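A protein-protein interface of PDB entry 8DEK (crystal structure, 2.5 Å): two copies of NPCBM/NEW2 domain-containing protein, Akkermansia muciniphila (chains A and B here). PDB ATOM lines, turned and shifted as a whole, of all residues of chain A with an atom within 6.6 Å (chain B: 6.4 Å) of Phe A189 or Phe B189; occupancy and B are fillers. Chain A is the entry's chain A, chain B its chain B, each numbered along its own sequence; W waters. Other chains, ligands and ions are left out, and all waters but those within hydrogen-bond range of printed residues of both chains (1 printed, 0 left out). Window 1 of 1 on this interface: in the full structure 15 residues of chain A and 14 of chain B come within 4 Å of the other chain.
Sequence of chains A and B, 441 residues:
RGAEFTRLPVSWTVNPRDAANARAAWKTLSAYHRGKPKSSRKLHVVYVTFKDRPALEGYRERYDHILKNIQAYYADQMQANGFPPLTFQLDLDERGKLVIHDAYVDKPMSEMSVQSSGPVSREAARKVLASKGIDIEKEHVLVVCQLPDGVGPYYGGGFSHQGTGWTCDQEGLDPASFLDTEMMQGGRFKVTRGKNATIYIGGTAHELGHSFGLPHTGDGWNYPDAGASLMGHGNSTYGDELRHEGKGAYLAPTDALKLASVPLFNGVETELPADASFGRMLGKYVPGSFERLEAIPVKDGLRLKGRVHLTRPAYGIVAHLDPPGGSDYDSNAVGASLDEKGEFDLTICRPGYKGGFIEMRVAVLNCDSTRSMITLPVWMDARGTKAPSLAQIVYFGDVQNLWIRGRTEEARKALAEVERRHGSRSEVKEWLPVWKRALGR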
ATOM      1  N   ASP A 149      25.381  16.356   9.963  1.00  0.00           N
ATOM      2  CA  ASP A 149      24.262  16.682  10.832  1.00  0.00           C
ATOM      3  C   ASP A 149      23.190  15.603  10.728  1.00  0.00           C
ATOM      4  O   ASP A 149      23.028  14.950   9.693  1.00  0.00           O
ATOM      5  CB  ASP A 149      23.677  18.044  10.459  1.00  0.00           C
ATOM      6  CG  ASP A 149      24.240  19.169  11.303  1.00  0.00           C
ATOM      7  OD1 ASP A 149      23.959  19.199  12.521  1.00  0.00           O
ATOM      8  OD2 ASP A 149      24.958  20.027  10.749  1.00  0.00           O
ATOM      9  N   TYR A 154      26.732  16.405  18.876  1.00  0.00           N
ATOM     10  CA  TYR A 154      27.138  17.725  19.354  1.00  0.00           C
ATOM     11  C   TYR A 154      26.750  17.785  20.828  1.00  0.00           C
ATOM     12  O   TYR A 154      25.627  18.163  21.169  1.00  0.00           O
ATOM     13  CB  TYR A 154      26.480  18.850  18.550  1.00  0.00           C
ATOM     14  CG  TYR A 154      26.762  18.806  17.065  1.00  0.00           C
ATOM     15  CD1 TYR A 154      25.974  18.045  16.210  1.00  0.00           C
ATOM     16  CD2 TYR A 154      27.813  19.529  16.517  1.00  0.00           C
ATOM     17  CE1 TYR A 154      26.225  18.004  14.853  1.00  0.00           C
ATOM     18  CE2 TYR A 154      28.073  19.495  15.159  1.00  0.00           C
ATOM     19  CZ  TYR A 154      27.275  18.731  14.331  1.00  0.00           C
ATOM     20  OH  TYR A 154      27.529  18.693  12.980  1.00  0.00           O
ATOM     21  N   MET A 183      26.061  33.394   1.343  1.00  0.00           N
ATOM     22  CA  MET A 183      25.015  32.503   1.826  1.00  0.00           C
ATOM     23  C   MET A 183      25.351  31.060   1.471  1.00  0.00           C
ATOM     24  O   MET A 183      25.923  30.784   0.413  1.00  0.00           O
ATOM     25  CB  MET A 183      23.668  32.912   1.232  1.00  0.00           C
ATOM     26  CG  MET A 183      23.071  34.165   1.870  1.00  0.00           C
ATOM     27  SD  MET A 183      22.434  33.971   3.550  1.00  0.00           S
ATOM     28  CE  MET A 183      21.889  32.260   3.546  1.00  0.00           C
ATOM     29  N   MET A 184      24.989  30.137   2.366  1.00  0.00           N
ATOM     30  CA  MET A 184      25.249  28.721   2.115  1.00  0.00           C
ATOM     31  C   MET A 184      24.384  28.194   0.977  1.00  0.00           C
ATOM     32  O   MET A 184      24.898  27.616   0.013  1.00  0.00           O
ATOM     33  CB  MET A 184      25.019  27.915   3.394  1.00  0.00           C
ATOM     34  CG  MET A 184      26.083  28.129   4.460  1.00  0.00           C
ATOM     35  SD  MET A 184      26.718  26.588   5.146  1.00  0.00           S
ATOM     36  CE  MET A 184      27.841  26.077   3.850  1.00  0.00           C
ATOM     37  N   GLN A 185      23.068  28.376   1.071  1.00  0.00           N
ATOM     38  CA  GLN A 185      22.165  27.902   0.029  1.00  0.00           C
ATOM     39  C   GLN A 185      21.867  26.412   0.131  1.00  0.00           C
ATOM     40  O   GLN A 185      22.751  25.609   0.445  1.00  0.00           O
ATOM     41  N   GLY A 186      20.616  26.040  -0.135  1.00  0.00           N
ATOM     42  CA  GLY A 186      20.207  24.652  -0.225  1.00  0.00           C
ATOM     43  C   GLY A 186      20.103  23.922   1.092  1.00  0.00           C
ATOM     44  O   GLY A 186      19.900  22.703   1.094  1.00  0.00           O
ATOM     45  N   GLY A 187      20.233  24.626   2.211  1.00  0.00           N
ATOM     46  CA  GLY A 187      20.139  24.010   3.519  1.00  0.00           C
ATOM     47  C   GLY A 187      18.871  24.400   4.245  1.00  0.00           C
ATOM     48  O   GLY A 187      18.239  25.404   3.900  1.00  0.00           O
ATOM     49  N   ARG A 188      18.478  23.611   5.247  1.00  0.00           N
ATOM     50  CA  ARG A 188      17.297  23.960   6.028  1.00  0.00           C
ATOM     51  C   ARG A 188      17.497  25.268   6.782  1.00  0.00           C
ATOM     52  O   ARG A 188      16.546  26.039   6.956  1.00  0.00           O
ATOM     53  CB  ARG A 188      16.957  22.831   7.002  1.00  0.00           C
ATOM     54  CG  ARG A 188      15.675  23.054   7.784  1.00  0.00           C
ATOM     55  CD  ARG A 188      15.178  21.775   8.440  1.00  0.00           C
ATOM     56  NE  ARG A 188      16.250  21.021   9.077  1.00  0.00           N
ATOM     57  CZ  ARG A 188      16.548  21.088  10.367  1.00  0.00           C
ATOM     58  NH1 ARG A 188      15.887  21.889  11.189  1.00  0.00           N
ATOM     59  NH2 ARG A 188      17.535  20.336  10.846  1.00  0.00           N
ATOM     60  N   PHE A 189      18.722  25.540   7.224  1.00  0.00           N
ATOM     61  CA  PHE A 189      19.048  26.749   7.971  1.00  0.00           C
ATOM     62  C   PHE A 189      19.606  27.792   7.010  1.00  0.00           C
ATOM     63  O   PHE A 189      20.714  27.636   6.486  1.00  0.00           O
ATOM     64  CB  PHE A 189      20.033  26.432   9.091  1.00  0.00           C
ATOM     65  CG  PHE A 189      19.418  25.678  10.229  1.00  0.00           C
ATOM     66  CD1 PHE A 189      19.277  24.301  10.166  1.00  0.00           C
ATOM     67  CD2 PHE A 189      18.973  26.343  11.359  1.00  0.00           C
ATOM     68  CE1 PHE A 189      18.704  23.601  11.207  1.00  0.00           C
ATOM     69  CE2 PHE A 189      18.400  25.647  12.405  1.00  0.00           C
ATOM     70  CZ  PHE A 189      18.267  24.274  12.329  1.00  0.00           C
ATOM     71  N   LYS A 190      18.833  28.850   6.779  1.00  0.00           N
ATOM     72  CA  LYS A 190      19.205  29.921   5.857  1.00  0.00           C
ATOM     73  C   LYS A 190      20.148  30.884   6.570  1.00  0.00           C
ATOM     74  O   LYS A 190      19.725  31.877   7.166  1.00  0.00           O
ATOM     75  CB  LYS A 190      17.964  30.635   5.339  1.00  0.00           C
ATOM     76  CG  LYS A 190      16.908  29.701   4.774  1.00  0.00           C
ATOM     77  CD  LYS A 190      17.502  28.762   3.737  1.00  0.00           C
ATOM     78  CE  LYS A 190      16.417  28.023   2.975  1.00  0.00           C
ATOM     79  NZ  LYS A 190      16.932  27.473   1.691  1.00  0.00           N
ATOM     80  N   VAL A 191      21.446  30.594   6.501  1.00  0.00           N
ATOM     81  CA  VAL A 191      22.453  31.347   7.240  1.00  0.00           C
ATOM     82  C   VAL A 191      23.714  31.421   6.391  1.00  0.00           C
ATOM     83  O   VAL A 191      23.962  30.563   5.540  1.00  0.00           O
ATOM     84  CB  VAL A 191      22.761  30.714   8.619  1.00  0.00           C
ATOM     85  CG1 VAL A 191      21.673  31.059   9.630  1.00  0.00           C
ATOM     86  CG2 VAL A 191      22.917  29.209   8.489  1.00  0.00           C
ATOM     87  N   THR A 192      24.514  32.455   6.635  1.00  0.00           N
ATOM     88  CA  THR A 192      25.732  32.665   5.867  1.00  0.00           C
ATOM     89  C   THR A 192      26.771  31.600   6.219  1.00  0.00           C
ATOM     90  O   THR A 192      26.639  30.857   7.196  1.00  0.00           O
ATOM     91  CB  THR A 192      26.295  34.064   6.120  1.00  0.00           C
ATOM     92  OG1 THR A 192      26.674  34.193   7.496  1.00  0.00           O
ATOM     93  CG2 THR A 192      25.255  35.125   5.786  1.00  0.00           C
ATOM     94  N   ASN A 196      27.431  29.877   9.746  1.00  0.00           N
ATOM     95  CA  ASN A 196      27.549  28.427   9.856  1.00  0.00           C
ATOM     96  C   ASN A 196      28.797  28.034  10.636  1.00  0.00           C
ATOM     97  O   ASN A 196      28.755  27.124  11.472  1.00  0.00           O
ATOM     98  CB  ASN A 196      27.555  27.797   8.463  1.00  0.00           C
ATOM     99  CG  ASN A 196      27.659  26.284   8.505  1.00  0.00           C
ATOM    100  OD1 ASN A 196      26.727  25.597   8.925  1.00  0.00           O
ATOM    101  ND2 ASN A 196      28.791  25.755   8.055  1.00  0.00           N
ATOM    102  N   ILE A 199      28.250  28.742  14.365  1.00  0.00           N
ATOM    103  CA  ILE A 199      27.499  27.699  15.057  1.00  0.00           C
ATOM    104  C   ILE A 199      28.395  26.500  15.346  1.00  0.00           C
ATOM    105  O   ILE A 199      28.338  25.913  16.434  1.00  0.00           O
ATOM    106  CB  ILE A 199      26.257  27.305  14.238  1.00  0.00           C
ATOM    107  CG1 ILE A 199      25.307  28.497  14.106  1.00  0.00           C
ATOM    108  CG2 ILE A 199      25.536  26.137  14.885  1.00  0.00           C
ATOM    109  CD1 ILE A 199      24.202  28.290  13.094  1.00  0.00           C
ATOM    110  N   ASN A 235      26.617  30.321  22.007  1.00  0.00           N
ATOM    111  CA  ASN A 235      27.117  29.314  21.077  1.00  0.00           C
ATOM    112  C   ASN A 235      26.790  29.671  19.634  1.00  0.00           C
ATOM    113  O   ASN A 235      27.514  29.270  18.714  1.00  0.00           O
ATOM    114  CB  ASN A 235      26.530  27.947  21.426  1.00  0.00           C
ATOM    115  CG  ASN A 235      25.054  27.848  21.092  1.00  0.00           C
ATOM    116  OD1 ASN A 235      24.212  28.444  21.765  1.00  0.00           O
ATOM    117  ND2 ASN A 235      24.734  27.099  20.042  1.00  0.00           N
ATOM    118  N   ASP B 149      19.482  15.930   7.005  1.00  0.00           N
ATOM    119  CA  ASP B 149      20.261  17.138   6.770  1.00  0.00           C
ATOM    120  C   ASP B 149      21.643  16.791   6.228  1.00  0.00           C
ATOM    121  O   ASP B 149      22.193  15.720   6.499  1.00  0.00           O
ATOM    122  CB  ASP B 149      20.396  17.951   8.058  1.00  0.00           C
ATOM    123  CG  ASP B 149      19.085  18.567   8.498  1.00  0.00           C
ATOM    124  OD1 ASP B 149      18.044  18.253   7.883  1.00  0.00           O
ATOM    125  OD2 ASP B 149      19.095  19.365   9.456  1.00  0.00           O
ATOM    126  N   TYR B 154      16.647  21.547   0.615  1.00  0.00           N
ATOM    127  CA  TYR B 154      15.699  22.543   1.110  1.00  0.00           C
ATOM    128  C   TYR B 154      15.799  23.716   0.139  1.00  0.00           C
ATOM    129  O   TYR B 154      16.622  24.617   0.317  1.00  0.00           O
ATOM    130  CB  TYR B 154      16.010  22.959   2.545  1.00  0.00           C
ATOM    131  CG  TYR B 154      15.956  21.824   3.542  1.00  0.00           C
ATOM    132  CD1 TYR B 154      17.061  21.014   3.764  1.00  0.00           C
ATOM    133  CD2 TYR B 154      14.796  21.561   4.261  1.00  0.00           C
ATOM    134  CE1 TYR B 154      17.017  19.974   4.676  1.00  0.00           C
ATOM    135  CE2 TYR B 154      14.740  20.524   5.173  1.00  0.00           C
ATOM    136  CZ  TYR B 154      15.853  19.735   5.377  1.00  0.00           C
ATOM    137  OH  TYR B 154      15.802  18.702   6.285  1.00  0.00           O
ATOM    138  N   MET B 184      15.577  20.418  22.034  1.00  0.00           N
ATOM    139  CA  MET B 184      16.096  19.296  21.265  1.00  0.00           C
ATOM    140  C   MET B 184      17.454  18.889  21.826  1.00  0.00           C
ATOM    141  O   MET B 184      18.229  19.725  22.299  1.00  0.00           O
ATOM    142  CB  MET B 184      16.188  19.650  19.781  1.00  0.00           C
ATOM    143  CG  MET B 184      14.839  19.569  19.084  1.00  0.00           C
ATOM    144  SD  MET B 184      14.845  18.725  17.490  1.00  0.00           S
ATOM    145  CE  MET B 184      13.083  18.528  17.225  1.00  0.00           C
ATOM    146  N   GLY B 187      21.924  18.082  19.155  1.00  0.00           N
ATOM    147  CA  GLY B 187      22.106  18.693  17.853  1.00  0.00           C
ATOM    148  C   GLY B 187      23.009  19.908  17.864  1.00  0.00           C
ATOM    149  O   GLY B 187      23.219  20.529  18.910  1.00  0.00           O
ATOM    150  N   ARG B 188      23.551  20.252  16.692  1.00  0.00           N
ATOM    151  CA  ARG B 188      24.422  21.418  16.581  1.00  0.00           C
ATOM    152  C   ARG B 188      23.684  22.707  16.912  1.00  0.00           C
ATOM    153  O   ARG B 188      24.282  23.645  17.454  1.00  0.00           O
ATOM    154  CB  ARG B 188      25.020  21.497  15.176  1.00  0.00           C
ATOM    155  CG  ARG B 188      26.058  22.592  15.016  1.00  0.00           C
ATOM    156  CD  ARG B 188      26.798  22.488  13.692  1.00  0.00           C
ATOM    157  NE  ARG B 188      25.927  22.099  12.589  1.00  0.00           N
ATOM    158  CZ  ARG B 188      25.590  22.897  11.584  1.00  0.00           C
ATOM    159  NH1 ARG B 188      26.015  24.149  11.523  1.00  0.00           N
ATOM    160  NH2 ARG B 188      24.812  22.426  10.615  1.00  0.00           N
ATOM    161  N   PHE B 189      22.393  22.771  16.606  1.00  0.00           N
ATOM    162  CA  PHE B 189      21.589  23.959  16.864  1.00  0.00           C
ATOM    163  C   PHE B 189      20.911  23.790  18.216  1.00  0.00           C
ATOM    164  O   PHE B 189      20.010  22.960  18.368  1.00  0.00           O
ATOM    165  CB  PHE B 189      20.569  24.163  15.749  1.00  0.00           C
ATOM    166  CG  PHE B 189      21.156  24.063  14.372  1.00  0.00           C
ATOM    167  CD1 PHE B 189      21.732  25.169  13.769  1.00  0.00           C
ATOM    168  CD2 PHE B 189      21.162  22.855  13.693  1.00  0.00           C
ATOM    169  CE1 PHE B 189      22.282  25.077  12.507  1.00  0.00           C
ATOM    170  CE2 PHE B 189      21.715  22.755  12.432  1.00  0.00           C
ATOM    171  CZ  PHE B 189      22.274  23.869  11.838  1.00  0.00           C
ATOM    172  N   LYS B 190      21.342  24.580  19.196  1.00  0.00           N
ATOM    173  CA  LYS B 190      20.803  24.481  20.551  1.00  0.00           C
ATOM    174  C   LYS B 190      19.469  25.209  20.541  1.00  0.00           C
ATOM    175  O   LYS B 190      19.376  26.399  20.847  1.00  0.00           O
ATOM    176  CB  LYS B 190      21.770  25.075  21.566  1.00  0.00           C
ATOM    177  CG  LYS B 190      23.152  24.440  21.550  1.00  0.00           C
ATOM    178  CD  LYS B 190      23.067  22.935  21.364  1.00  0.00           C
ATOM    179  CE  LYS B 190      24.378  22.260  21.712  1.00  0.00           C
ATOM    180  NZ  LYS B 190      24.206  20.795  21.905  1.00  0.00           N
ATOM    181  N   VAL B 191      18.416  24.477  20.179  1.00  0.00           N
ATOM    182  CA  VAL B 191      17.110  25.073  19.934  1.00  0.00           C
ATOM    183  C   VAL B 191      16.024  24.091  20.350  1.00  0.00           C
ATOM    184  O   VAL B 191      16.238  22.877  20.401  1.00  0.00           O
ATOM    185  CB  VAL B 191      16.963  25.477  18.449  1.00  0.00           C
ATOM    186  CG1 VAL B 191      16.610  24.270  17.582  1.00  0.00           C
ATOM    187  CG2 VAL B 191      15.971  26.603  18.308  1.00  0.00           C
ATOM    188  N   THR B 192      14.848  24.632  20.663  1.00  0.00           N
ATOM    189  CA  THR B 192      13.730  23.828  21.133  1.00  0.00           C
ATOM    190  C   THR B 192      13.152  22.973  20.005  1.00  0.00           C
ATOM    191  O   THR B 192      13.433  23.172  18.819  1.00  0.00           O
ATOM    192  CB  THR B 192      12.631  24.719  21.708  1.00  0.00           C
ATOM    193  OG1 THR B 192      11.723  25.088  20.663  1.00  0.00           O
ATOM    194  CG2 THR B 192      13.227  25.982  22.310  1.00  0.00           C
ATOM    195  N   ASN B 196      12.301  23.956  15.989  1.00  0.00           N
ATOM    196  CA  ASN B 196      12.753  23.031  14.954  1.00  0.00           C
ATOM    197  C   ASN B 196      11.642  22.755  13.950  1.00  0.00           C
ATOM    198  O   ASN B 196      11.893  22.676  12.741  1.00  0.00           O
ATOM    199  CB  ASN B 196      13.247  21.728  15.581  1.00  0.00           C
ATOM    200  CG  ASN B 196      13.847  20.784  14.556  1.00  0.00           C
ATOM    201  OD1 ASN B 196      13.294  19.721  14.274  1.00  0.00           O
ATOM    202  ND2 ASN B 196      14.985  21.171  13.988  1.00  0.00           N
ATOM    203  N   ILE B 199      11.384  25.818  11.802  1.00  0.00           N
ATOM    204  CA  ILE B 199      12.377  25.862  10.731  1.00  0.00           C
ATOM    205  C   ILE B 199      11.941  24.982   9.567  1.00  0.00           C
ATOM    206  O   ILE B 199      12.072  25.363   8.397  1.00  0.00           O
ATOM    207  CB  ILE B 199      13.764  25.438  11.258  1.00  0.00           C
ATOM    208  CG1 ILE B 199      14.197  26.259  12.479  1.00  0.00           C
ATOM    209  CG2 ILE B 199      14.806  25.575  10.167  1.00  0.00           C
ATOM    210  CD1 ILE B 199      13.841  27.719  12.426  1.00  0.00           C
ATOM    211  N   ASN B 235      11.281  32.687   7.573  1.00  0.00           N
ATOM    212  CA  ASN B 235      11.294  31.230   7.490  1.00  0.00           C
ATOM    213  C   ASN B 235      11.682  30.591   8.817  1.00  0.00           C
ATOM    214  O   ASN B 235      11.273  29.459   9.103  1.00  0.00           O
ATOM    215  CB  ASN B 235      12.250  30.775   6.389  1.00  0.00           C
ATOM    216  CG  ASN B 235      13.701  31.055   6.725  1.00  0.00           C
ATOM    217  OD1 ASN B 235      14.165  32.192   6.626  1.00  0.00           O
ATOM    218  ND2 ASN B 235      14.425  30.018   7.132  1.00  0.00           N
HETATM  219  O   HOH W   1      14.061  27.107   7.239  1.00  0.00           O
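The backbone NH (N) of Tyr B154 lies within hydrogen-bond range of the backbone carbonyl oxygen (O) of Gly A186, at 3.5 Å.
The side-chain amino group (NZ) of Lys B190 is in hydrogen-bond range of the backbone carbonyl oxygen (O) of Tyr A154, at 3.1 Å.
The backbone carbonyl oxygen (O) of Asp A149 sits close to the backbone carbonyl oxygen (O) of Asp B149 (3.4 Å).
The backbone carbonyl oxygen (O) of Tyr B154 is in hydrogen-bond range of the side-chain amino group (NZ) of Lys A190, 3.2 Å away.
The side-chain amide oxygen of Asn A196 lies within hydrogen-bond range of the guanidinium group of Arg B188 (3.1 Å).
ND2 of Asn B196 lies close to NH1 of Arg A188 (3.0 Å).
NH2 of Arg B188 lies within salt-bridge range of OD2 of Asp A149.
OD2 of Asp B149 lies within salt-bridge range of NE of Arg A188.
NZ of Lys B190 lies within hydrogen-bond range of O of Gly B187, 3.2 Å away.
The backbone carbonyl oxygen (O) of Gly A187 is in hydrogen-bond range of the side-chain amino group (NZ) of Lys A190, at 3.3 Å.
The side-chain sulfur (SD) of Met B184 lies close to the side-chain amide oxygen (OD1) of Asn B196, 3.7 Å away.
OH of Tyr B154 lies within hydrogen-bond range of OD1 of Asp B149, at 2.8 Å.
The side-chain sulfur of Met A184 lies close to the side-chain amide nitrogen of Asn A196 (3.7 Å).
Among the printed residues, merely in contact across the chains: Tyr A154 with Gly B187, Tyr A154 with Arg B188, Gly A187 with Tyr B154, Arg A188 with Tyr B154, Arg A188 with Ile B199, Phe A189 with Phe B189, Lys A190 with Asn B235, Ile A199 with Arg B188, Ile A199 with Phe B189 and Asn A235 with Lys B190.
Gln A185 touches none of the printed residues of chain B.
Phe A189 touches one residue of chain B.
Of the printed residues of chain B, Asn A196 touches Arg B188 (3.1 Å).
Printed residues of chain B within 4 Å of Asn A235: Lys B190.
Met B184 touches none of the printed residues of chain A.
Of the printed residues of chain A, Asn B196 touches Arg A188.
The nearest printed residue of chain B that does not touch Asn A196 is Phe B189 (5.6 Å).
Hydrophobic or aromatic side chains of chain A that line the printed part of chain B: Tyr A154, Phe A189 and Ile A199.
Hydrophobic or aromatic side chains of chain B that line the printed part of chain A: Tyr B154, Phe B189 and Ile B199.
Along chain B the printed residues that touch a printed residue of chain A span positions 149 to 235.
Among the printed residues, 18 pairs touch across the chains.
Among the printed residues, Asp or Glu carboxylates within 4 Å of a Lys or Arg side-chain nitrogen of the other chain: Asp A149 with Arg B188 (2.4 Å) and Arg A188 with Asp B149 (2.3 Å).
Tyr A154 touches Gly B187, and with the chains exchanged Gly A187 touches Tyr B154.
Arg A188 touches Ile B199, and with the chains exchanged Ile A199 touches Arg B188.
Phe A189 touches its own counterpart, Phe B189.
Lys A190 touches Asn B235, and with the chains exchanged Asn A235 touches Lys B190.
12 positions are printed for both chains.
Water W1 lies within hydrogen-bond range of the backbone carbonyl oxygen of Arg A188 (2.7 Å), the backbone carbonyl oxygen of Ile B199 (2.9 Å) and the side-chain amide nitrogen of Asn B235 (2.9 Å).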
